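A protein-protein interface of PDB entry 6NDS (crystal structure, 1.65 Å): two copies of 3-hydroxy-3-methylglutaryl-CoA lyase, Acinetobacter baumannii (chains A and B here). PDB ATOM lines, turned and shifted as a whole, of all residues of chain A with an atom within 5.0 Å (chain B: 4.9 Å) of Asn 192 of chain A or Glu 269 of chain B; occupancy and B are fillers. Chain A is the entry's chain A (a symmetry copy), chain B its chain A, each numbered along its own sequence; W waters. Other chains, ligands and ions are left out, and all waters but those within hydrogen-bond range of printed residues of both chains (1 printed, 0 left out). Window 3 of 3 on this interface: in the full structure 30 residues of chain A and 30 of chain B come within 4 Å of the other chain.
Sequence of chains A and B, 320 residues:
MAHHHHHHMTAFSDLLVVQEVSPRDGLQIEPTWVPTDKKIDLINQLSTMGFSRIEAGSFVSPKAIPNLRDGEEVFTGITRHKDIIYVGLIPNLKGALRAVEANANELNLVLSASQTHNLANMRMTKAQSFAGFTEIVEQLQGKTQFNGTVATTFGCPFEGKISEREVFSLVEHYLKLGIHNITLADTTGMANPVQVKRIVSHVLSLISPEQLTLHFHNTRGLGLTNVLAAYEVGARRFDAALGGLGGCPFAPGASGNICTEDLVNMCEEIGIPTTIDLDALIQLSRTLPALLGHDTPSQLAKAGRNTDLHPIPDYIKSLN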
ATOM      1  N   MET A 190      28.958   9.572  11.092  1.00  0.00           N
ATOM      2  CA  MET A 190      27.662   9.493  10.439  1.00  0.00           C
ATOM      3  C   MET A 190      27.746   9.499   8.915  1.00  0.00           C
ATOM      4  O   MET A 190      26.713   9.300   8.256  1.00  0.00           O
ATOM      5  CB  MET A 190      26.776  10.646  10.923  1.00  0.00           C
ATOM      6  CG  MET A 190      26.462  10.528  12.432  1.00  0.00           C
ATOM      7  SD  MET A 190      25.546  11.931  13.079  1.00  0.00           S
ATOM      8  CE  MET A 190      23.910  11.641  12.417  1.00  0.00           C
ATOM      9  N   ALA A 191      28.932   9.700   8.339  1.00  0.00           N
ATOM     10  CA  ALA A 191      29.062   9.858   6.891  1.00  0.00           C
ATOM     11  C   ALA A 191      28.964   8.523   6.146  1.00  0.00           C
ATOM     12  O   ALA A 191      29.286   7.458   6.681  1.00  0.00           O
ATOM     13  CB  ALA A 191      30.396  10.521   6.537  1.00  0.00           C
ATOM     14  N   ASN A 192      28.505   8.588   4.900  1.00  0.00           N
ATOM     15  CA  ASN A 192      28.507   7.444   3.997  1.00  0.00           C
ATOM     16  C   ASN A 192      29.206   7.838   2.702  1.00  0.00           C
ATOM     17  O   ASN A 192      29.331   9.026   2.393  1.00  0.00           O
ATOM     18  CB  ASN A 192      27.082   6.937   3.711  1.00  0.00           C
ATOM     19  CG  ASN A 192      26.281   7.883   2.840  1.00  0.00           C
ATOM     20  OD1 ASN A 192      26.484   7.953   1.618  1.00  0.00           O
ATOM     21  ND2 ASN A 192      25.339   8.592   3.451  1.00  0.00           N
ATOM     22  N   PRO A 193      29.682   6.857   1.926  1.00  0.00           N
ATOM     23  CA  PRO A 193      30.539   7.194   0.767  1.00  0.00           C
ATOM     24  C   PRO A 193      29.876   8.048  -0.304  1.00  0.00           C
ATOM     25  O   PRO A 193      30.561   8.882  -0.909  1.00  0.00           O
ATOM     26  CB  PRO A 193      30.924   5.816   0.216  1.00  0.00           C
ATOM     27  CG  PRO A 193      30.832   4.905   1.386  1.00  0.00           C
ATOM     28  CD  PRO A 193      29.732   5.424   2.268  1.00  0.00           C
ATOM     29  N   VAL A 194      28.586   7.851  -0.595  1.00  0.00           N
ATOM     30  CA  VAL A 194      27.938   8.664  -1.624  1.00  0.00           C
ATOM     31  C   VAL A 194      27.857  10.113  -1.168  1.00  0.00           C
ATOM     32  O   VAL A 194      28.166  11.044  -1.926  1.00  0.00           O
ATOM     33  CB  VAL A 194      26.552   8.100  -1.970  1.00  0.00           C
ATOM     34  CG1 VAL A 194      25.791   9.082  -2.856  1.00  0.00           C
ATOM     35  CG2 VAL A 194      26.713   6.772  -2.676  1.00  0.00           C
ATOM     36  N   GLN A 195      27.448  10.317   0.084  1.00  0.00           N
ATOM     37  CA  GLN A 195      27.415  11.654   0.667  1.00  0.00           C
ATOM     38  C   GLN A 195      28.798  12.288   0.668  1.00  0.00           C
ATOM     39  O   GLN A 195      28.951  13.475   0.348  1.00  0.00           O
ATOM     40  CB  GLN A 195      26.866  11.562   2.088  1.00  0.00           C
ATOM     41  CG  GLN A 195      26.963  12.823   2.926  1.00  0.00           C
ATOM     42  CD  GLN A 195      26.816  12.489   4.405  1.00  0.00           C
ATOM     43  OE1 GLN A 195      27.256  11.433   4.845  1.00  0.00           O
ATOM     44  NE2 GLN A 195      26.190  13.380   5.168  1.00  0.00           N
ATOM     45  N   VAL A 196      29.820  11.504   1.016  1.00  0.00           N
ATOM     46  CA  VAL A 196      31.186  12.019   1.018  1.00  0.00           C
ATOM     47  C   VAL A 196      31.587  12.487  -0.375  1.00  0.00           C
ATOM     48  O   VAL A 196      32.165  13.566  -0.538  1.00  0.00           O
ATOM     49  CB  VAL A 196      32.152  10.953   1.557  1.00  0.00           C
ATOM     50  CG1 VAL A 196      33.601  11.329   1.234  1.00  0.00           C
ATOM     51  CG2 VAL A 196      31.954  10.796   3.070  1.00  0.00           C
ATOM     52  N   LEU A 222      32.438   2.760   8.722  1.00  0.00           N
ATOM     53  CA  LEU A 222      32.608   3.222   7.348  1.00  0.00           C
ATOM     54  C   LEU A 222      33.820   4.119   7.155  1.00  0.00           C
ATOM     55  O   LEU A 222      34.007   4.661   6.055  1.00  0.00           O
ATOM     56  CB  LEU A 222      31.347   3.957   6.884  1.00  0.00           C
ATOM     57  CG  LEU A 222      30.115   3.060   6.860  1.00  0.00           C
ATOM     58  CD1 LEU A 222      28.921   3.863   6.396  1.00  0.00           C
ATOM     59  CD2 LEU A 222      30.354   1.852   5.974  1.00  0.00           C
ATOM     60  N   ASN A 226      34.933   5.607   3.577  1.00  0.00           N
ATOM     61  CA  ASN A 226      34.767   7.032   3.308  1.00  0.00           C
ATOM     62  C   ASN A 226      36.073   7.681   2.860  1.00  0.00           C
ATOM     63  O   ASN A 226      36.053   8.603   2.033  1.00  0.00           O
ATOM     64  CB  ASN A 226      34.214   7.738   4.553  1.00  0.00           C
ATOM     65  CG  ASN A 226      32.774   7.392   4.833  1.00  0.00           C
ATOM     66  OD1 ASN A 226      31.995   7.079   3.920  1.00  0.00           O
ATOM     67  ND2 ASN A 226      32.372   7.478   6.120  1.00  0.00           N
ATOM     68  N   ASN B 265      23.724  -1.611   7.296  1.00  0.00           N
ATOM     69  CA  ASN B 265      23.682  -0.162   7.517  1.00  0.00           C
ATOM     70  C   ASN B 265      24.374   0.587   6.387  1.00  0.00           C
ATOM     71  O   ASN B 265      23.882   1.619   5.922  1.00  0.00           O
ATOM     72  CB  ASN B 265      24.330   0.199   8.860  1.00  0.00           C
ATOM     73  CG  ASN B 265      24.318   1.697   9.117  1.00  0.00           C
ATOM     74  OD1 ASN B 265      23.266   2.284   9.408  1.00  0.00           O
ATOM     75  ND2 ASN B 265      25.488   2.335   8.983  1.00  0.00           N
ATOM     76  N   MET B 266      25.524   0.082   5.931  1.00  0.00           N
ATOM     77  CA  MET B 266      26.208   0.716   4.807  1.00  0.00           C
ATOM     78  C   MET B 266      25.295   0.805   3.586  1.00  0.00           C
ATOM     79  O   MET B 266      25.177   1.866   2.952  1.00  0.00           O
ATOM     80  CB  MET B 266      27.474  -0.071   4.461  1.00  0.00           C
ATOM     81  CG  MET B 266      28.197   0.545   3.258  1.00  0.00           C
ATOM     82  SD  MET B 266      29.794  -0.199   2.863  1.00  0.00           S
ATOM     83  CE  MET B 266      29.300  -1.720   2.051  1.00  0.00           C
ATOM     84  N   CYS B 267      24.643  -0.311   3.241  1.00  0.00           N
ATOM     85  CA  CYS B 267      23.703  -0.331   2.119  1.00  0.00           C
ATOM     86  C   CYS B 267      22.560   0.642   2.338  1.00  0.00           C
ATOM     87  O   CYS B 267      22.179   1.381   1.425  1.00  0.00           O
ATOM     88  CB  CYS B 267      23.149  -1.739   1.923  1.00  0.00           C
ATOM     89  SG  CYS B 267      24.363  -2.938   1.353  1.00  0.00           S
ATOM     90  N   GLU B 268      21.980   0.635   3.548  1.00  0.00           N
ATOM     91  CA  GLU B 268      20.822   1.473   3.828  1.00  0.00           C
ATOM     92  C   GLU B 268      21.167   2.956   3.705  1.00  0.00           C
ATOM     93  O   GLU B 268      20.390   3.742   3.150  1.00  0.00           O
ATOM     94  CB  GLU B 268      20.275   1.124   5.220  1.00  0.00           C
ATOM     95  CG  GLU B 268      18.958   1.783   5.554  1.00  0.00           C
ATOM     96  CD  GLU B 268      17.982   0.876   6.301  1.00  0.00           C
ATOM     97  OE1 GLU B 268      18.008  -0.370   6.122  1.00  0.00           O
ATOM     98  OE2 GLU B 268      17.155   1.437   7.041  1.00  0.00           O
ATOM     99  N   GLU B 269      22.352   3.352   4.183  1.00  0.00           N
ATOM    100  CA  GLU B 269      22.758   4.752   4.105  1.00  0.00           C
ATOM    101  C   GLU B 269      23.121   5.175   2.683  1.00  0.00           C
ATOM    102  O   GLU B 269      22.863   6.319   2.294  1.00  0.00           O
ATOM    103  CB  GLU B 269      23.932   5.002   5.052  1.00  0.00           C
ATOM    104  CG  GLU B 269      23.529   4.916   6.517  1.00  0.00           C
ATOM    105  CD  GLU B 269      22.455   5.934   6.869  1.00  0.00           C
ATOM    106  OE1 GLU B 269      22.715   7.148   6.727  1.00  0.00           O
ATOM    107  OE2 GLU B 269      21.334   5.523   7.255  1.00  0.00           O
ATOM    108  N   ILE B 270      23.752   4.285   1.910  1.00  0.00           N
ATOM    109  CA  ILE B 270      24.146   4.623   0.543  1.00  0.00           C
ATOM    110  C   ILE B 270      22.944   4.655  -0.381  1.00  0.00           C
ATOM    111  O   ILE B 270      22.895   5.462  -1.317  1.00  0.00           O
ATOM    112  CB  ILE B 270      25.193   3.607   0.047  1.00  0.00           C
ATOM    113  CG1 ILE B 270      26.543   3.849   0.717  1.00  0.00           C
ATOM    114  CG2 ILE B 270      25.351   3.656  -1.466  1.00  0.00           C
ATOM    115  CD1 ILE B 270      27.541   2.725   0.370  1.00  0.00           C
ATOM    116  N   GLY B 271      21.962   3.800  -0.138  1.00  0.00           N
ATOM    117  CA  GLY B 271      20.850   3.622  -1.038  1.00  0.00           C
ATOM    118  C   GLY B 271      20.882   2.332  -1.832  1.00  0.00           C
ATOM    119  O   GLY B 271      20.140   2.218  -2.822  1.00  0.00           O
ATOM    120  N   ARG B 305      22.240   3.185  14.952  1.00  0.00           N
ATOM    121  CA  ARG B 305      22.228   3.814  13.636  1.00  0.00           C
ATOM    122  C   ARG B 305      22.202   5.340  13.766  1.00  0.00           C
ATOM    123  O   ARG B 305      22.022   5.899  14.853  1.00  0.00           O
ATOM    124  CB  ARG B 305      21.028   3.330  12.833  1.00  0.00           C
ATOM    125  CG  ARG B 305      19.706   3.703  13.482  1.00  0.00           C
ATOM    126  CD  ARG B 305      18.557   3.014  12.766  1.00  0.00           C
ATOM    127  NE  ARG B 305      18.653   3.251  11.329  1.00  0.00           N
ATOM    128  CZ  ARG B 305      17.971   2.571  10.417  1.00  0.00           C
ATOM    129  NH1 ARG B 305      17.132   1.614  10.801  1.00  0.00           N
ATOM    130  NH2 ARG B 305      18.132   2.852   9.124  1.00  0.00           N
ATOM    131  N   ASN B 306      22.377   6.020  12.620  1.00  0.00           N
ATOM    132  CA  ASN B 306      22.451   7.485  12.602  1.00  0.00           C
ATOM    133  C   ASN B 306      21.238   8.129  13.260  1.00  0.00           C
ATOM    134  O   ASN B 306      21.359   9.173  13.918  1.00  0.00           O
ATOM    135  CB  ASN B 306      22.549   7.992  11.162  1.00  0.00           C
ATOM    136  CG  ASN B 306      23.958   7.919  10.587  1.00  0.00           C
ATOM    137  OD1 ASN B 306      24.798   7.150  11.042  1.00  0.00           O
ATOM    138  ND2 ASN B 306      24.213   8.732   9.567  1.00  0.00           N
HETATM  139  O   HOH W   1      24.940   8.443   6.220  1.00  0.00           O
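The side-chain amide nitrogen of Asn 306 of chain B sits at hydrogen-bond distance from the backbone carbonyl oxygen of Met 190 of chain A (2.9 Å).
Of the 9 printed residues of chain B, 4 touch a printed residue of chain A. Among the printed residues, no Asp or Glu carboxylate lies within 4 Å of a Lys or Arg side-chain nitrogen of the other chain.
OD1 of Asn 192 of chain A lies within hydrogen-bond range of N of Val 194 of chain A (3.1 Å). N of Gln 195 of chain A lies within hydrogen-bond range of OD1 of Asn 192 of chain A (3.0 Å). The side-chain amide nitrogen of Asn 226 of chain A sits close to the backbone carbonyl oxygen of Leu 222 of chain A, 3.3 Å away.
Water W1 lies within hydrogen-bond range of OE1 of Glu 269 of chain B (2.6 Å), ND2 of Asn 192 of chain A (2.8 Å), O of Met 190 of chain A (2.8 Å) and ND2 of Asn 306 of chain B (3.4 Å).
Printed residues of chain B within 4 Å of Met 190 of chain A: Asn 306. Asn 192 of chain A touches one residue of chain B. Of the printed residues of chain B, Pro 193 of chain A touches Ile 270 (3.9 Å). Printed residues of chain B within 4 Å of Leu 222 of chain A: Met 266 (3.7 Å). Of chain A, only Asn 192 comes within 4 Å of Glu 269 of chain B. Of the printed residues of chain A, Ile 270 of chain B touches Pro 193 and Val 194. Of the printed residues of chain A, Asn 306 of chain B touches Met 190. The nearest residue of chain B that does not touch Asn 192 of chain A is Ile 270 of chain B (4.2 Å). The nearest printed residue of chain A that does not touch Asn 306 of chain B is Ala 191 of chain A (5.0 Å).
Asn 192 of chain A touches Glu 269 of chain B (ND2 to O, 3.6 Å). CD of Pro 193 of chain A touches CG1 of Ile 270 of chain B, at 3.9 Å. Val 194 of chain A touches Ile 270 of chain B (CG2 to CG2, 3.6 Å). Met 266 of chain B touches Leu 222 of chain A.
No position is printed for both chains.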
